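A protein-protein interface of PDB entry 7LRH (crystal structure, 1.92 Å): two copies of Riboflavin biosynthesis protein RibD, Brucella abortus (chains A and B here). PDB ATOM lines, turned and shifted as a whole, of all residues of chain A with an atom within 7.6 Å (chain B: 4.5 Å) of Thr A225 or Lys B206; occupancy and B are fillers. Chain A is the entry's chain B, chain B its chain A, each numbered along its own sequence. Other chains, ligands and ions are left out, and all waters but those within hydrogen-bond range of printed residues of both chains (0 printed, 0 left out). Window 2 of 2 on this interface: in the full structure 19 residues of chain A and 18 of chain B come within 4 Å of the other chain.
Asn A224 touches Lys B206, but with the chains exchanged Lys A206 does not touch Asn B224 (8.6 Å).
Positions printed for both chains: 205, 206, 222 and 224.
Of the 4 pairs that touch across the chains among the printed residues, none has its exchanged pair printed and touching as well.
Printed residues of chain B within 4 Å of Val A222: Leu B208 (3.5 Å).
Printed residues of chain B within 4 Å of Arg A223: Lys B206.
Printed residues of chain B within 4 Å of Asn A224: Lys B206.
Of chain B, only Lys B206 (3.5 Å) comes within 4 Å of Thr A225.
Lys B206 touches three residues of chain A.
Ile B207 touches none of the printed residues of chain A.
Of the printed residues of chain A, Leu B208 touches Val A222.
The nearest printed residue of chain B that does not touch Thr A225 is Ile B207 (7.3 Å).
The nearest printed residue of chain B that does not touch Val A222 is Lys B206 (4.6 Å).
CD2 of Leu B208 touches CG1 of Val A222 (3.5 Å).
Arg A223 touches Lys B206 (O to NZ, 3.8 Å).
N of Lys B206 is in hydrogen-bond range of O of Val B222.
N of Leu B208 sits at hydrogen-bond distance from O of Glu B220, at 2.7 Å.
The backbone carbonyl oxygen (O) of Glu A204 sits at hydrogen-bond distance from the backbone NH (N) of Asn A224 (2.9 Å).
The backbone NH (N) of Phe A205 sits close to the side-chain amide nitrogen (ND2) of Asn A224 (3.4 Å).
N of Val A222 lies within hydrogen-bond range of O of Lys A206, at 3.0 Å.
The side-chain amide oxygen (OD1) of Asn A224 sits at hydrogen-bond distance from the side-chain amino group (NZ) of Lys A206 (2.8 Å).
NZ of Lys B206 is in hydrogen-bond range of O of Asn A224 (3.5 Å).
NZ of Lys B206 is in salt-bridge range of O of Thr A225, at 3.5 Å.
Hydrophobic or aromatic side chains of chain A within 4 Å of the printed part of chain B: Val A222.
Of the 8 printed residues of chain B, 2 touch a printed residue of chain A.
Printed residues of chain B that touch a printed residue of chain A: Lys B206 and Leu B208.
Hydrophobic or aromatic side chains of chain B within 4 Å of the printed part of chain A: Leu B208.
Along chain B the printed residues that touch a printed residue of chain A span positions 206 to 208.
Among the printed residues, no Asp or Glu carboxylate lies within 4 Å of a Lys or Arg side-chain nitrogen of the other chain.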
ATOM      1  N   ASP A 175      10.406  30.867  -8.040  1.00  0.00           N
ATOM      2  CA  ASP A 175       9.754  30.777  -6.731  1.00  0.00           C
ATOM      3  C   ASP A 175      10.055  29.461  -6.012  1.00  0.00           C
ATOM      4  O   ASP A 175      10.205  29.426  -4.785  1.00  0.00           O
ATOM      5  CB  ASP A 175       8.235  30.934  -6.887  1.00  0.00           C
ATOM      6  CG  ASP A 175       7.856  32.247  -7.560  1.00  0.00           C
ATOM      7  OD1 ASP A 175       8.128  33.313  -6.960  1.00  0.00           O
ATOM      8  OD2 ASP A 175       7.330  32.199  -8.688  1.00  0.00           O
ATOM      9  N   GLU A 204      18.990  32.744  -1.311  1.00  0.00           N
ATOM     10  CA  GLU A 204      17.574  33.044  -1.528  1.00  0.00           C
ATOM     11  C   GLU A 204      16.592  31.906  -1.213  1.00  0.00           C
ATOM     12  O   GLU A 204      15.390  32.105  -1.413  1.00  0.00           O
ATOM     13  CB  GLU A 204      17.324  33.513  -2.978  1.00  0.00           C
ATOM     14  CG  GLU A 204      18.246  34.623  -3.502  1.00  0.00           C
ATOM     15  CD  GLU A 204      18.598  34.478  -5.004  1.00  0.00           C
ATOM     16  OE1 GLU A 204      17.685  34.367  -5.864  1.00  0.00           O
ATOM     17  OE2 GLU A 204      19.804  34.468  -5.335  1.00  0.00           O
ATOM     18  N   PHE A 205      17.045  30.710  -0.812  1.00  0.00           N
ATOM     19  CA  PHE A 205      16.166  29.549  -0.705  1.00  0.00           C
ATOM     20  C   PHE A 205      16.339  28.807   0.619  1.00  0.00           C
ATOM     21  O   PHE A 205      17.423  28.797   1.206  1.00  0.00           O
ATOM     22  CB  PHE A 205      16.406  28.565  -1.876  1.00  0.00           C
ATOM     23  CG  PHE A 205      15.960  29.083  -3.239  1.00  0.00           C
ATOM     24  CD1 PHE A 205      16.799  29.881  -4.011  1.00  0.00           C
ATOM     25  CD2 PHE A 205      14.738  28.731  -3.765  1.00  0.00           C
ATOM     26  CE1 PHE A 205      16.400  30.335  -5.261  1.00  0.00           C
ATOM     27  CE2 PHE A 205      14.341  29.188  -5.019  1.00  0.00           C
ATOM     28  CZ  PHE A 205      15.159  29.982  -5.761  1.00  0.00           C
ATOM     29  N   LYS A 206      15.251  28.148   1.057  1.00  0.00           N
ATOM     30  CA  LYS A 206      15.197  27.189   2.159  1.00  0.00           C
ATOM     31  C   LYS A 206      14.801  25.821   1.635  1.00  0.00           C
ATOM     32  O   LYS A 206      13.931  25.725   0.771  1.00  0.00           O
ATOM     33  CB  LYS A 206      14.170  27.528   3.266  1.00  0.00           C
ATOM     34  CG  LYS A 206      14.233  28.827   4.011  1.00  0.00           C
ATOM     35  CD  LYS A 206      15.383  28.933   4.998  1.00  0.00           C
ATOM     36  CE  LYS A 206      15.662  30.413   5.070  1.00  0.00           C
ATOM     37  NZ  LYS A 206      16.788  30.813   4.202  1.00  0.00           N
ATOM     38  N   VAL A 222      12.150  26.566  -1.511  1.00  0.00           N
ATOM     39  CA  VAL A 222      11.272  27.706  -1.784  1.00  0.00           C
ATOM     40  C   VAL A 222      12.017  29.002  -1.492  1.00  0.00           C
ATOM     41  O   VAL A 222      12.826  29.060  -0.560  1.00  0.00           O
ATOM     42  CB  VAL A 222       9.981  27.596  -0.937  1.00  0.00           C
ATOM     43  CG1 VAL A 222       9.109  28.844  -1.050  1.00  0.00           C
ATOM     44  CG2 VAL A 222       9.201  26.374  -1.377  1.00  0.00           C
ATOM     45  N   ARG A 223      11.674  30.073  -2.213  1.00  0.00           N
ATOM     46  CA  ARG A 223      12.350  31.343  -1.997  1.00  0.00           C
ATOM     47  C   ARG A 223      11.935  31.947  -0.666  1.00  0.00           C
ATOM     48  O   ARG A 223      10.765  31.891  -0.286  1.00  0.00           O
ATOM     49  CB  ARG A 223      12.048  32.327  -3.121  1.00  0.00           C
ATOM     50  CG  ARG A 223      12.850  33.621  -2.952  1.00  0.00           C
ATOM     51  CD  ARG A 223      13.073  34.336  -4.242  1.00  0.00           C
ATOM     52  NE  ARG A 223      11.814  34.567  -4.942  1.00  0.00           N
ATOM     53  CZ  ARG A 223      11.715  35.128  -6.153  1.00  0.00           C
ATOM     54  NH1 ARG A 223      12.798  35.519  -6.804  1.00  0.00           N
ATOM     55  NH2 ARG A 223      10.526  35.310  -6.704  1.00  0.00           N
ATOM     56  N   ASN A 224      12.906  32.567   0.016  1.00  0.00           N
ATOM     57  CA  ASN A 224      12.761  32.983   1.411  1.00  0.00           C
ATOM     58  C   ASN A 224      11.593  33.922   1.655  1.00  0.00           C
ATOM     59  O   ASN A 224      10.963  33.869   2.724  1.00  0.00           O
ATOM     60  CB  ASN A 224      14.058  33.614   1.877  1.00  0.00           C
ATOM     61  CG  ASN A 224      15.113  32.594   2.021  1.00  0.00           C
ATOM     62  OD1 ASN A 224      14.801  31.462   2.352  1.00  0.00           O
ATOM     63  ND2 ASN A 224      16.358  32.947   1.721  1.00  0.00           N
ATOM     64  N   THR A 225      11.305  34.803   0.708  1.00  0.00           N
ATOM     65  CA  THR A 225      10.336  35.871   0.936  1.00  0.00           C
ATOM     66  C   THR A 225       8.922  35.364   1.238  1.00  0.00           C
ATOM     67  O   THR A 225       8.558  35.117   2.398  1.00  0.00           O
ATOM     68  CB  THR A 225      10.294  36.794  -0.279  1.00  0.00           C
ATOM     69  OG1 THR A 225       9.708  36.092  -1.392  1.00  0.00           O
ATOM     70  CG2 THR A 225      11.727  37.258  -0.636  1.00  0.00           C
ATOM     71  OXT THR A 225       8.110  35.189   0.320  1.00  0.00           O
ATOM     72  N   PHE B 205       1.046  29.452   8.587  1.00  0.00           N
ATOM     73  CA  PHE B 205       1.380  28.857   7.297  1.00  0.00           C
ATOM     74  C   PHE B 205       1.455  29.920   6.218  1.00  0.00           C
ATOM     75  O   PHE B 205       0.789  30.964   6.298  1.00  0.00           O
ATOM     76  CB  PHE B 205       0.345  27.752   6.858  1.00  0.00           C
ATOM     77  CG  PHE B 205       0.507  26.441   7.599  1.00  0.00           C
ATOM     78  CD1 PHE B 205       1.379  25.480   7.138  1.00  0.00           C
ATOM     79  CD2 PHE B 205      -0.192  26.202   8.777  1.00  0.00           C
ATOM     80  CE1 PHE B 205       1.575  24.306   7.824  1.00  0.00           C
ATOM     81  CE2 PHE B 205      -0.012  25.004   9.491  1.00  0.00           C
ATOM     82  CZ  PHE B 205       0.898  24.054   9.017  1.00  0.00           C
ATOM     83  N   LYS B 206       2.271  29.656   5.190  1.00  0.00           N
ATOM     84  CA  LYS B 206       2.234  30.472   3.984  1.00  0.00           C
ATOM     85  C   LYS B 206       1.992  29.598   2.762  1.00  0.00           C
ATOM     86  O   LYS B 206       2.563  28.518   2.637  1.00  0.00           O
ATOM     87  CB  LYS B 206       3.529  31.302   3.824  1.00  0.00           C
ATOM     88  CG  LYS B 206       4.755  30.511   3.588  1.00  0.00           C
ATOM     89  CD  LYS B 206       5.970  31.456   3.361  1.00  0.00           C
ATOM     90  CE  LYS B 206       7.264  30.701   3.052  1.00  0.00           C
ATOM     91  NZ  LYS B 206       8.306  31.660   2.560  1.00  0.00           N
ATOM     92  N   ILE B 207       1.178  30.109   1.839  1.00  0.00           N
ATOM     93  CA  ILE B 207       0.844  29.389   0.607  1.00  0.00           C
ATOM     94  C   ILE B 207       2.067  29.267  -0.298  1.00  0.00           C
ATOM     95  O   ILE B 207       2.852  30.210  -0.444  1.00  0.00           O
ATOM     96  CB  ILE B 207      -0.314  30.072  -0.133  1.00  0.00           C
ATOM     97  CG1 ILE B 207      -0.741  29.209  -1.318  1.00  0.00           C
ATOM     98  CG2 ILE B 207       0.046  31.481  -0.588  1.00  0.00           C
ATOM     99  CD1 ILE B 207      -2.230  29.063  -1.414  1.00  0.00           C
ATOM    100  N   LEU B 208       2.222  28.100  -0.923  1.00  0.00           N
ATOM    101  CA  LEU B 208       3.325  27.781  -1.824  1.00  0.00           C
ATOM    102  C   LEU B 208       2.912  27.685  -3.277  1.00  0.00           C
ATOM    103  O   LEU B 208       3.574  28.267  -4.156  1.00  0.00           O
ATOM    104  CB  LEU B 208       3.899  26.418  -1.414  1.00  0.00           C
ATOM    105  CG  LEU B 208       4.931  26.449  -0.328  1.00  0.00           C
ATOM    106  CD1 LEU B 208       5.562  25.063  -0.227  1.00  0.00           C
ATOM    107  CD2 LEU B 208       5.881  27.562  -0.731  1.00  0.00           C
ATOM    108  N   GLU B 220      -1.148  24.157  -1.598  1.00  0.00           N
ATOM    109  CA  GLU B 220      -0.021  23.700  -0.784  1.00  0.00           C
ATOM    110  C   GLU B 220       0.504  24.847   0.076  1.00  0.00           C
ATOM    111  O   GLU B 220       0.669  25.959  -0.410  1.00  0.00           O
ATOM    112  CB  GLU B 220       1.152  23.215  -1.644  1.00  0.00           C
ATOM    113  CG  GLU B 220       0.944  21.976  -2.461  1.00  0.00           C
ATOM    114  CD  GLU B 220       2.270  21.402  -3.024  1.00  0.00           C
ATOM    115  OE1 GLU B 220       3.355  22.092  -2.998  1.00  0.00           O
ATOM    116  OE2 GLU B 220       2.217  20.247  -3.506  1.00  0.00           O
ATOM    117  N   TYR B 221       0.795  24.565   1.340  1.00  0.00           N
ATOM    118  CA  TYR B 221       1.301  25.524   2.312  1.00  0.00           C
ATOM    119  C   TYR B 221       2.509  24.944   3.055  1.00  0.00           C
ATOM    120  O   TYR B 221       2.626  23.725   3.230  1.00  0.00           O
ATOM    121  CB  TYR B 221       0.240  25.871   3.387  1.00  0.00           C
ATOM    122  CG  TYR B 221      -1.074  26.301   2.856  1.00  0.00           C
ATOM    123  CD1 TYR B 221      -2.028  25.369   2.487  1.00  0.00           C
ATOM    124  CD2 TYR B 221      -1.388  27.642   2.738  1.00  0.00           C
ATOM    125  CE1 TYR B 221      -3.259  25.774   1.976  1.00  0.00           C
ATOM    126  CE2 TYR B 221      -2.648  28.043   2.257  1.00  0.00           C
ATOM    127  CZ  TYR B 221      -3.548  27.102   1.873  1.00  0.00           C
ATOM    128  OH  TYR B 221      -4.773  27.468   1.370  1.00  0.00           O
ATOM    129  N   VAL B 222       3.396  25.833   3.533  1.00  0.00           N
ATOM    130  CA  VAL B 222       4.465  25.418   4.421  1.00  0.00           C
ATOM    131  C   VAL B 222       4.396  26.264   5.678  1.00  0.00           C
ATOM    132  O   VAL B 222       3.997  27.442   5.636  1.00  0.00           O
ATOM    133  CB  VAL B 222       5.850  25.555   3.731  1.00  0.00           C
ATOM    134  CG1 VAL B 222       6.049  27.013   3.336  1.00  0.00           C
ATOM    135  CG2 VAL B 222       6.939  25.115   4.653  1.00  0.00           C
ATOM    136  N   ASN B 224       5.324  28.701   8.661  1.00  0.00           N
ATOM    137  CA  ASN B 224       6.034  29.968   8.638  1.00  0.00           C
ATOM    138  C   ASN B 224       7.445  29.785   9.164  1.00  0.00           C
ATOM    139  O   ASN B 224       7.689  29.030  10.115  1.00  0.00           O
ATOM    140  CB  ASN B 224       5.333  31.027   9.478  1.00  0.00           C
ATOM    141  CG  ASN B 224       4.147  31.614   8.791  1.00  0.00           C
ATOM    142  OD1 ASN B 224       4.109  31.733   7.556  1.00  0.00           O
ATOM    143  ND2 ASN B 224       3.149  32.018   9.580  1.00  0.00           N
